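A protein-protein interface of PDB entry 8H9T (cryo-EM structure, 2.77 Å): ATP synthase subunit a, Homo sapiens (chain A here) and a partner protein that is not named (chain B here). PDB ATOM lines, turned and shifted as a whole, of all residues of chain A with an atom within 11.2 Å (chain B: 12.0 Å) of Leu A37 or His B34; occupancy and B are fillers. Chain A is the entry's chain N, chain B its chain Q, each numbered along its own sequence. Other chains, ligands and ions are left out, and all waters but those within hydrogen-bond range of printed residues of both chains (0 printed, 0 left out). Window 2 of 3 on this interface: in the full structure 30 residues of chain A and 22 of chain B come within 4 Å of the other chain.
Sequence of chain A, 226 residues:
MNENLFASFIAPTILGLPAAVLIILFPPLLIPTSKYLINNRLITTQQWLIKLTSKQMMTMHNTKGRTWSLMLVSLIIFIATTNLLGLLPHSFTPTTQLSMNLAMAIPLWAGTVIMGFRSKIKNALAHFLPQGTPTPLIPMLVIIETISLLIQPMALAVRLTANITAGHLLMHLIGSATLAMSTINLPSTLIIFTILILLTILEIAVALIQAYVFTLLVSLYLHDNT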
ATOM      1  N   THR A  33      30.882  22.037  -5.968  1.00  0.00           N
ATOM      2  CA  THR A  33      29.508  21.682  -6.274  1.00  0.00           C
ATOM      3  C   THR A  33      28.998  20.697  -5.238  1.00  0.00           C
ATOM      4  O   THR A  33      29.775  20.025  -4.561  1.00  0.00           O
ATOM      5  CB  THR A  33      29.402  21.074  -7.664  1.00  0.00           C
ATOM      6  OG1 THR A  33      30.263  19.936  -7.741  1.00  0.00           O
ATOM      7  CG2 THR A  33      29.837  22.072  -8.696  1.00  0.00           C
ATOM      8  N   SER A  34      27.677  20.606  -5.120  1.00  0.00           N
ATOM      9  CA  SER A  34      27.101  19.718  -4.123  1.00  0.00           C
ATOM     10  C   SER A  34      25.708  19.296  -4.554  1.00  0.00           C
ATOM     11  O   SER A  34      25.020  20.020  -5.275  1.00  0.00           O
ATOM     12  CB  SER A  34      27.041  20.386  -2.750  1.00  0.00           C
ATOM     13  OG  SER A  34      25.899  21.214  -2.653  1.00  0.00           O
ATOM     14  N   LYS A  35      25.304  18.117  -4.090  1.00  0.00           N
ATOM     15  CA  LYS A  35      23.976  17.579  -4.337  1.00  0.00           C
ATOM     16  C   LYS A  35      22.960  18.002  -3.290  1.00  0.00           C
ATOM     17  O   LYS A  35      21.774  17.711  -3.453  1.00  0.00           O
ATOM     18  CB  LYS A  35      24.023  16.053  -4.377  1.00  0.00           C
ATOM     19  CG  LYS A  35      24.796  15.490  -5.540  1.00  0.00           C
ATOM     20  CD  LYS A  35      24.063  15.731  -6.840  1.00  0.00           C
ATOM     21  CE  LYS A  35      24.804  15.105  -8.005  1.00  0.00           C
ATOM     22  NZ  LYS A  35      25.133  13.680  -7.747  1.00  0.00           N
ATOM     23  N   TYR A  36      23.389  18.676  -2.230  1.00  0.00           N
ATOM     24  CA  TYR A  36      22.500  18.995  -1.128  1.00  0.00           C
ATOM     25  C   TYR A  36      21.451  20.008  -1.558  1.00  0.00           C
ATOM     26  O   TYR A  36      21.407  20.466  -2.699  1.00  0.00           O
ATOM     27  CB  TYR A  36      23.287  19.539   0.055  1.00  0.00           C
ATOM     28  CG  TYR A  36      24.048  18.496   0.810  1.00  0.00           C
ATOM     29  CD1 TYR A  36      24.811  18.838   1.908  1.00  0.00           C
ATOM     30  CD2 TYR A  36      24.006  17.170   0.425  1.00  0.00           C
ATOM     31  CE1 TYR A  36      25.510  17.891   2.603  1.00  0.00           C
ATOM     32  CE2 TYR A  36      24.700  16.213   1.114  1.00  0.00           C
ATOM     33  CZ  TYR A  36      25.452  16.578   2.204  1.00  0.00           C
ATOM     34  OH  TYR A  36      26.154  15.624   2.901  1.00  0.00           O
ATOM     35  N   LEU A  37      20.591  20.358  -0.615  1.00  0.00           N
ATOM     36  CA  LEU A  37      19.571  21.370  -0.817  1.00  0.00           C
ATOM     37  C   LEU A  37      19.823  22.625  -0.012  1.00  0.00           C
ATOM     38  O   LEU A  37      19.471  23.716  -0.452  1.00  0.00           O
ATOM     39  CB  LEU A  37      18.200  20.814  -0.448  1.00  0.00           C
ATOM     40  CG  LEU A  37      17.046  21.412  -1.234  1.00  0.00           C
ATOM     41  CD1 LEU A  37      17.233  21.110  -2.691  1.00  0.00           C
ATOM     42  CD2 LEU A  37      15.750  20.839  -0.741  1.00  0.00           C
ATOM     43  N   ILE A  38      20.418  22.491   1.161  1.00  0.00           N
ATOM     44  CA  ILE A  38      20.773  23.628   2.000  1.00  0.00           C
ATOM     45  C   ILE A  38      22.258  23.484   2.306  1.00  0.00           C
ATOM     46  O   ILE A  38      22.652  22.831   3.275  1.00  0.00           O
ATOM     47  CB  ILE A  38      19.938  23.688   3.276  1.00  0.00           C
ATOM     48  CG1 ILE A  38      18.465  23.798   2.914  1.00  0.00           C
ATOM     49  CG2 ILE A  38      20.357  24.867   4.124  1.00  0.00           C
ATOM     50  CD1 ILE A  38      18.148  25.025   2.110  1.00  0.00           C
ATOM     51  N   ASN A  39      23.092  24.105   1.480  1.00  0.00           N
ATOM     52  CA  ASN A  39      24.536  23.958   1.531  1.00  0.00           C
ATOM     53  C   ASN A  39      25.187  25.247   2.017  1.00  0.00           C
ATOM     54  O   ASN A  39      24.515  26.203   2.405  1.00  0.00           O
ATOM     55  CB  ASN A  39      25.051  23.526   0.166  1.00  0.00           C
ATOM     56  CG  ASN A  39      24.539  24.402  -0.928  1.00  0.00           C
ATOM     57  OD1 ASN A  39      23.931  25.436  -0.671  1.00  0.00           O
ATOM     58  ND2 ASN A  39      24.739  23.981  -2.163  1.00  0.00           N
ATOM     59  N   ASN A  40      26.516  25.261   1.995  1.00  0.00           N
ATOM     60  CA  ASN A  40      27.286  26.290   2.675  1.00  0.00           C
ATOM     61  C   ASN A  40      27.051  27.662   2.049  1.00  0.00           C
ATOM     62  O   ASN A  40      26.367  27.809   1.040  1.00  0.00           O
ATOM     63  CB  ASN A  40      28.764  25.945   2.622  1.00  0.00           C
ATOM     64  CG  ASN A  40      29.178  25.480   1.265  1.00  0.00           C
ATOM     65  OD1 ASN A  40      29.044  26.208   0.293  1.00  0.00           O
ATOM     66  ND2 ASN A  40      29.658  24.252   1.176  1.00  0.00           N
ATOM     67  N   ARG A  41      27.634  28.681   2.675  1.00  0.00           N
ATOM     68  CA  ARG A  41      27.458  30.035   2.173  1.00  0.00           C
ATOM     69  C   ARG A  41      28.104  30.204   0.810  1.00  0.00           C
ATOM     70  O   ARG A  41      27.569  30.905  -0.057  1.00  0.00           O
ATOM     71  CB  ARG A  41      28.035  31.037   3.160  1.00  0.00           C
ATOM     72  CG  ARG A  41      27.146  31.315   4.330  1.00  0.00           C
ATOM     73  CD  ARG A  41      27.965  31.730   5.517  1.00  0.00           C
ATOM     74  NE  ARG A  41      27.235  32.629   6.394  1.00  0.00           N
ATOM     75  CZ  ARG A  41      27.698  33.068   7.557  1.00  0.00           C
ATOM     76  NH1 ARG A  41      28.892  32.690   7.982  1.00  0.00           N
ATOM     77  NH2 ARG A  41      26.970  33.888   8.294  1.00  0.00           N
ATOM     78  N   ILE A  43      28.686  28.010  -1.800  1.00  0.00           N
ATOM     79  CA  ILE A  43      27.911  27.506  -2.923  1.00  0.00           C
ATOM     80  C   ILE A  43      26.560  28.192  -2.997  1.00  0.00           C
ATOM     81  O   ILE A  43      25.995  28.332  -4.081  1.00  0.00           O
ATOM     82  CB  ILE A  43      27.761  25.984  -2.845  1.00  0.00           C
ATOM     83  CG1 ILE A  43      29.120  25.344  -2.632  1.00  0.00           C
ATOM     84  CG2 ILE A  43      27.198  25.460  -4.128  1.00  0.00           C
ATOM     85  CD1 ILE A  43      29.040  23.974  -2.050  1.00  0.00           C
ATOM     86  N   THR A  44      26.023  28.653  -1.868  1.00  0.00           N
ATOM     87  CA  THR A  44      24.790  29.432  -1.920  1.00  0.00           C
ATOM     88  C   THR A  44      24.972  30.668  -2.787  1.00  0.00           C
ATOM     89  O   THR A  44      24.220  30.891  -3.745  1.00  0.00           O
ATOM     90  CB  THR A  44      24.355  29.835  -0.515  1.00  0.00           C
ATOM     91  OG1 THR A  44      23.812  28.699   0.161  1.00  0.00           O
ATOM     92  CG2 THR A  44      23.303  30.909  -0.585  1.00  0.00           C
ATOM     93  N   THR A  45      25.988  31.473  -2.479  1.00  0.00           N
ATOM     94  CA  THR A  45      26.205  32.692  -3.242  1.00  0.00           C
ATOM     95  C   THR A  45      26.604  32.384  -4.674  1.00  0.00           C
ATOM     96  O   THR A  45      26.199  33.090  -5.602  1.00  0.00           O
ATOM     97  CB  THR A  45      27.266  33.545  -2.574  1.00  0.00           C
ATOM     98  OG1 THR A  45      26.881  33.793  -1.222  1.00  0.00           O
ATOM     99  CG2 THR A  45      27.379  34.856  -3.284  1.00  0.00           C
ATOM    100  N   GLN A  47      25.738  29.775  -6.533  1.00  0.00           N
ATOM    101  CA  GLN A  47      24.575  29.374  -7.300  1.00  0.00           C
ATOM    102  C   GLN A  47      23.651  30.548  -7.539  1.00  0.00           C
ATOM    103  O   GLN A  47      23.042  30.638  -8.607  1.00  0.00           O
ATOM    104  CB  GLN A  47      23.844  28.244  -6.591  1.00  0.00           C
ATOM    105  CG  GLN A  47      24.635  26.972  -6.590  1.00  0.00           C
ATOM    106  CD  GLN A  47      23.785  25.774  -6.322  1.00  0.00           C
ATOM    107  OE1 GLN A  47      24.164  24.652  -6.643  1.00  0.00           O
ATOM    108  NE2 GLN A  47      22.625  25.997  -5.731  1.00  0.00           N
ATOM    109  N   TRP A  48      23.549  31.472  -6.583  1.00  0.00           N
ATOM    110  CA  TRP A  48      22.778  32.677  -6.851  1.00  0.00           C
ATOM    111  C   TRP A  48      23.370  33.451  -8.016  1.00  0.00           C
ATOM    112  O   TRP A  48      22.642  33.907  -8.903  1.00  0.00           O
ATOM    113  CB  TRP A  48      22.706  33.564  -5.617  1.00  0.00           C
ATOM    114  CG  TRP A  48      21.880  34.763  -5.862  1.00  0.00           C
ATOM    115  CD1 TRP A  48      20.542  34.793  -6.065  1.00  0.00           C
ATOM    116  CD2 TRP A  48      22.332  36.114  -5.957  1.00  0.00           C
ATOM    117  NE1 TRP A  48      20.122  36.079  -6.274  1.00  0.00           N
ATOM    118  CE2 TRP A  48      21.207  36.910  -6.213  1.00  0.00           C
ATOM    119  CE3 TRP A  48      23.577  36.727  -5.849  1.00  0.00           C
ATOM    120  CZ2 TRP A  48      21.289  38.284  -6.361  1.00  0.00           C
ATOM    121  CZ3 TRP A  48      23.655  38.090  -5.994  1.00  0.00           C
ATOM    122  CH2 TRP A  48      22.521  38.854  -6.248  1.00  0.00           C
ATOM    123  N   LYS A  51      22.742  31.597 -11.318  1.00  0.00           N
ATOM    124  CA  LYS A  51      21.341  31.766 -11.671  1.00  0.00           C
ATOM    125  C   LYS A  51      21.104  33.135 -12.284  1.00  0.00           C
ATOM    126  O   LYS A  51      20.476  33.260 -13.344  1.00  0.00           O
ATOM    127  CB  LYS A  51      20.480  31.568 -10.427  1.00  0.00           C
ATOM    128  CG  LYS A  51      19.132  32.231 -10.480  1.00  0.00           C
ATOM    129  CD  LYS A  51      18.186  31.610  -9.462  1.00  0.00           C
ATOM    130  CE  LYS A  51      18.348  32.224  -8.088  1.00  0.00           C
ATOM    131  NZ  LYS A  51      18.044  33.680  -8.102  1.00  0.00           N
ATOM    132  N   MET B  28      29.572  23.017 -13.922  1.00  0.00           N
ATOM    133  CA  MET B  28      28.238  23.599 -14.031  1.00  0.00           C
ATOM    134  C   MET B  28      27.164  22.519 -14.039  1.00  0.00           C
ATOM    135  O   MET B  28      26.209  22.579 -13.261  1.00  0.00           O
ATOM    136  CB  MET B  28      28.130  24.449 -15.289  1.00  0.00           C
ATOM    137  CG  MET B  28      28.724  25.810 -15.190  1.00  0.00           C
ATOM    138  SD  MET B  28      27.946  26.777 -13.919  1.00  0.00           S
ATOM    139  CE  MET B  28      29.287  26.819 -12.755  1.00  0.00           C
ATOM    140  N   LEU B  29      27.314  21.517 -14.907  1.00  0.00           N
ATOM    141  CA  LEU B  29      26.320  20.460 -15.051  1.00  0.00           C
ATOM    142  C   LEU B  29      25.934  19.822 -13.732  1.00  0.00           C
ATOM    143  O   LEU B  29      24.887  19.178 -13.655  1.00  0.00           O
ATOM    144  CB  LEU B  29      26.844  19.379 -15.981  1.00  0.00           C
ATOM    145  CG  LEU B  29      26.390  19.550 -17.413  1.00  0.00           C
ATOM    146  CD1 LEU B  29      26.804  18.357 -18.221  1.00  0.00           C
ATOM    147  CD2 LEU B  29      24.904  19.692 -17.414  1.00  0.00           C
ATOM    148  N   ASN B  30      26.754  19.961 -12.704  1.00  0.00           N
ATOM    149  CA  ASN B  30      26.383  19.517 -11.376  1.00  0.00           C
ATOM    150  C   ASN B  30      25.663  20.593 -10.584  1.00  0.00           C
ATOM    151  O   ASN B  30      25.310  20.356  -9.428  1.00  0.00           O
ATOM    152  CB  ASN B  30      27.617  19.054 -10.612  1.00  0.00           C
ATOM    153  CG  ASN B  30      27.285  18.053  -9.543  1.00  0.00           C
ATOM    154  OD1 ASN B  30      26.490  17.146  -9.763  1.00  0.00           O
ATOM    155  ND2 ASN B  30      27.876  18.215  -8.369  1.00  0.00           N
ATOM    156  N   THR B  31      25.442  21.762 -11.167  1.00  0.00           N
ATOM    157  CA  THR B  31      24.662  22.821 -10.538  1.00  0.00           C
ATOM    158  C   THR B  31      23.272  22.808 -11.155  1.00  0.00           C
ATOM    159  O   THR B  31      23.105  23.152 -12.329  1.00  0.00           O
ATOM    160  CB  THR B  31      25.331  24.176 -10.723  1.00  0.00           C
ATOM    161  OG1 THR B  31      26.462  24.269  -9.857  1.00  0.00           O
ATOM    162  CG2 THR B  31      24.374  25.290 -10.398  1.00  0.00           C
ATOM    163  N   ASN B  32      22.275  22.410 -10.371  1.00  0.00           N
ATOM    164  CA  ASN B  32      20.909  22.308 -10.856  1.00  0.00           C
ATOM    165  C   ASN B  32      19.963  23.056  -9.934  1.00  0.00           C
ATOM    166  O   ASN B  32      20.099  23.004  -8.709  1.00  0.00           O
ATOM    167  CB  ASN B  32      20.477  20.860 -10.971  1.00  0.00           C
ATOM    168  CG  ASN B  32      21.221  20.125 -12.048  1.00  0.00           C
ATOM    169  OD1 ASN B  32      21.913  19.146 -11.785  1.00  0.00           O
ATOM    170  ND2 ASN B  32      21.092  20.601 -13.275  1.00  0.00           N
ATOM    171  N   TYR B  33      19.005  23.744 -10.536  1.00  0.00           N
ATOM    172  CA  TYR B  33      18.012  24.537  -9.826  1.00  0.00           C
ATOM    173  C   TYR B  33      16.678  23.813  -9.920  1.00  0.00           C
ATOM    174  O   TYR B  33      16.000  23.875 -10.947  1.00  0.00           O
ATOM    175  CB  TYR B  33      17.917  25.934 -10.418  1.00  0.00           C
ATOM    176  CG  TYR B  33      19.239  26.637 -10.486  1.00  0.00           C
ATOM    177  CD1 TYR B  33      19.712  27.347  -9.404  1.00  0.00           C
ATOM    178  CD2 TYR B  33      20.014  26.587 -11.627  1.00  0.00           C
ATOM    179  CE1 TYR B  33      20.910  27.987  -9.456  1.00  0.00           C
ATOM    180  CE2 TYR B  33      21.217  27.223 -11.685  1.00  0.00           C
ATOM    181  CZ  TYR B  33      21.658  27.923 -10.594  1.00  0.00           C
ATOM    182  OH  TYR B  33      22.861  28.571 -10.628  1.00  0.00           O
ATOM    183  N   HIS B  34      16.313  23.125  -8.844  1.00  0.00           N
ATOM    184  CA  HIS B  34      15.046  22.413  -8.801  1.00  0.00           C
ATOM    185  C   HIS B  34      13.883  23.388  -8.902  1.00  0.00           C
ATOM    186  O   HIS B  34      13.935  24.495  -8.361  1.00  0.00           O
ATOM    187  CB  HIS B  34      14.943  21.623  -7.507  1.00  0.00           C
ATOM    188  CG  HIS B  34      14.868  22.488  -6.294  1.00  0.00           C
ATOM    189  ND1 HIS B  34      13.718  23.149  -5.925  1.00  0.00           N
ATOM    190  CD2 HIS B  34      15.803  22.820  -5.378  1.00  0.00           C
ATOM    191  CE1 HIS B  34      13.946  23.843  -4.826  1.00  0.00           C
ATOM    192  NE2 HIS B  34      15.204  23.659  -4.473  1.00  0.00           N
ATOM    193  N   LEU B  35      12.829  22.969  -9.593  1.00  0.00           N
ATOM    194  CA  LEU B  35      11.639  23.795  -9.691  1.00  0.00           C
ATOM    195  C   LEU B  35      11.011  23.951  -8.311  1.00  0.00           C
ATOM    196  O   LEU B  35      11.057  23.022  -7.504  1.00  0.00           O
ATOM    197  CB  LEU B  35      10.638  23.178 -10.654  1.00  0.00           C
ATOM    198  CG  LEU B  35      11.199  22.954 -12.053  1.00  0.00           C
ATOM    199  CD1 LEU B  35      11.669  21.532 -12.206  1.00  0.00           C
ATOM    200  CD2 LEU B  35      10.162  23.279 -13.099  1.00  0.00           C
ATOM    201  N   PRO B  36      10.428  25.104  -8.009  1.00  0.00           N
ATOM    202  CA  PRO B  36       9.942  25.356  -6.656  1.00  0.00           C
ATOM    203  C   PRO B  36       8.848  24.376  -6.286  1.00  0.00           C
ATOM    204  O   PRO B  36       8.097  23.916  -7.158  1.00  0.00           O
ATOM    205  CB  PRO B  36       9.397  26.789  -6.733  1.00  0.00           C
ATOM    206  CG  PRO B  36       9.988  27.366  -7.961  1.00  0.00           C
ATOM    207  CD  PRO B  36      10.149  26.230  -8.908  1.00  0.00           C
ATOM    208  N   PRO B  37       8.727  24.026  -5.007  1.00  0.00           N
ATOM    209  CA  PRO B  37       7.651  23.122  -4.588  1.00  0.00           C
ATOM    210  C   PRO B  37       6.314  23.832  -4.723  1.00  0.00           C
ATOM    211  O   PRO B  37       6.080  24.866  -4.097  1.00  0.00           O
ATOM    212  CB  PRO B  37       7.996  22.813  -3.131  1.00  0.00           C
ATOM    213  CG  PRO B  37       8.765  23.981  -2.680  1.00  0.00           C
ATOM    214  CD  PRO B  37       9.488  24.547  -3.863  1.00  0.00           C
ATOM    215  N   SER B  38       5.433  23.292  -5.568  1.00  0.00           N
ATOM    216  CA  SER B  38       4.074  23.876  -5.721  1.00  0.00           C
ATOM    217  C   SER B  38       3.037  22.934  -5.099  1.00  0.00           C
ATOM    218  O   SER B  38       2.291  22.291  -5.864  1.00  0.00           O
ATOM    219  CB  SER B  38       3.767  24.152  -7.169  1.00  0.00           C
ATOM    220  OG  SER B  38       2.452  24.668  -7.316  1.00  0.00           O
ATOM    221  N   PRO B  39       2.954  22.821  -3.754  1.00  0.00           N
ATOM    222  CA  PRO B  39       2.023  21.891  -3.110  1.00  0.00           C
ATOM    223  C   PRO B  39       0.577  22.346  -3.339  1.00  0.00           C
ATOM    224  O   PRO B  39       0.087  23.113  -2.536  1.00  0.00           O
ATOM    225  CB  PRO B  39       2.381  21.991  -1.621  1.00  0.00           C
ATOM    226  CG  PRO B  39       2.970  23.376  -1.483  1.00  0.00           C
ATOM    227  CD  PRO B  39       3.721  23.600  -2.779  1.00  0.00           C
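The side-chain hydroxyl (OH) of Tyr B33 lies within hydrogen-bond range of the backbone NH (N) of Lys A51, at 3.1 Å. OH of Tyr B33 is in hydrogen-bond range of O of Gln A47 (2.9 Å). OG1 of Thr A33 is in hydrogen-bond range of ND2 of Asn B30 (3.0 Å).
Among the printed residues, pairs that only touch across the chains: Lys A35 with Asn B30, Leu A37 with His B34 and Gln A47 with Thr B31.
Leu A37 touches one residue of chain B. Of chain A, only Leu A37 comes within 4 Å of His B34. No residue of chain B comes within 4 Å of Ile A38. No residue of chain B comes within 4 Å of Asn A39. No residue of chain A comes within 4 Å of Leu B35. No residue of chain A comes within 4 Å of Pro B36. Printed residues of chain A within 4 Å of Thr B31: Gln A47 (3.8 Å). Printed residues of chain A within 4 Å of Tyr B33: Gln A47 (2.9 Å) and Lys A51 (3.1 Å). Printed residues of chain A within 4 Å of Asn B30: Thr A33 and Lys A35. Of the printed residues of chain B, Lys A35 touches Asn B30. Of the printed residues of chain B, Gln A47 touches Thr B31 and Tyr B33. Asn A40 touches none of the printed residues of chain B. The nearest residue of chain B that does not touch Leu A37 is Asn B32 (6.9 Å). The nearest residue of chain A that does not touch His B34 is Tyr A36 (6.6 Å). The nearest printed residue of chain B that does not touch Gln A47 is Asn B32 (4.7 Å).
Of the 12 printed residues of chain B, 4 touch a printed residue of chain A. Printed residues of chain B that touch a printed residue of chain A: Asn B30, Thr B31, Tyr B33 and His B34. Hydrophobic or aromatic side chains of chain A within 4 Å of the printed part of chain B: Leu A37. Among the printed residues, 6 pairs touch across the chains. Among the printed residues, no Asp or Glu carboxylate lies within 4 Å of a Lys or Arg side-chain nitrogen of the other chain.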
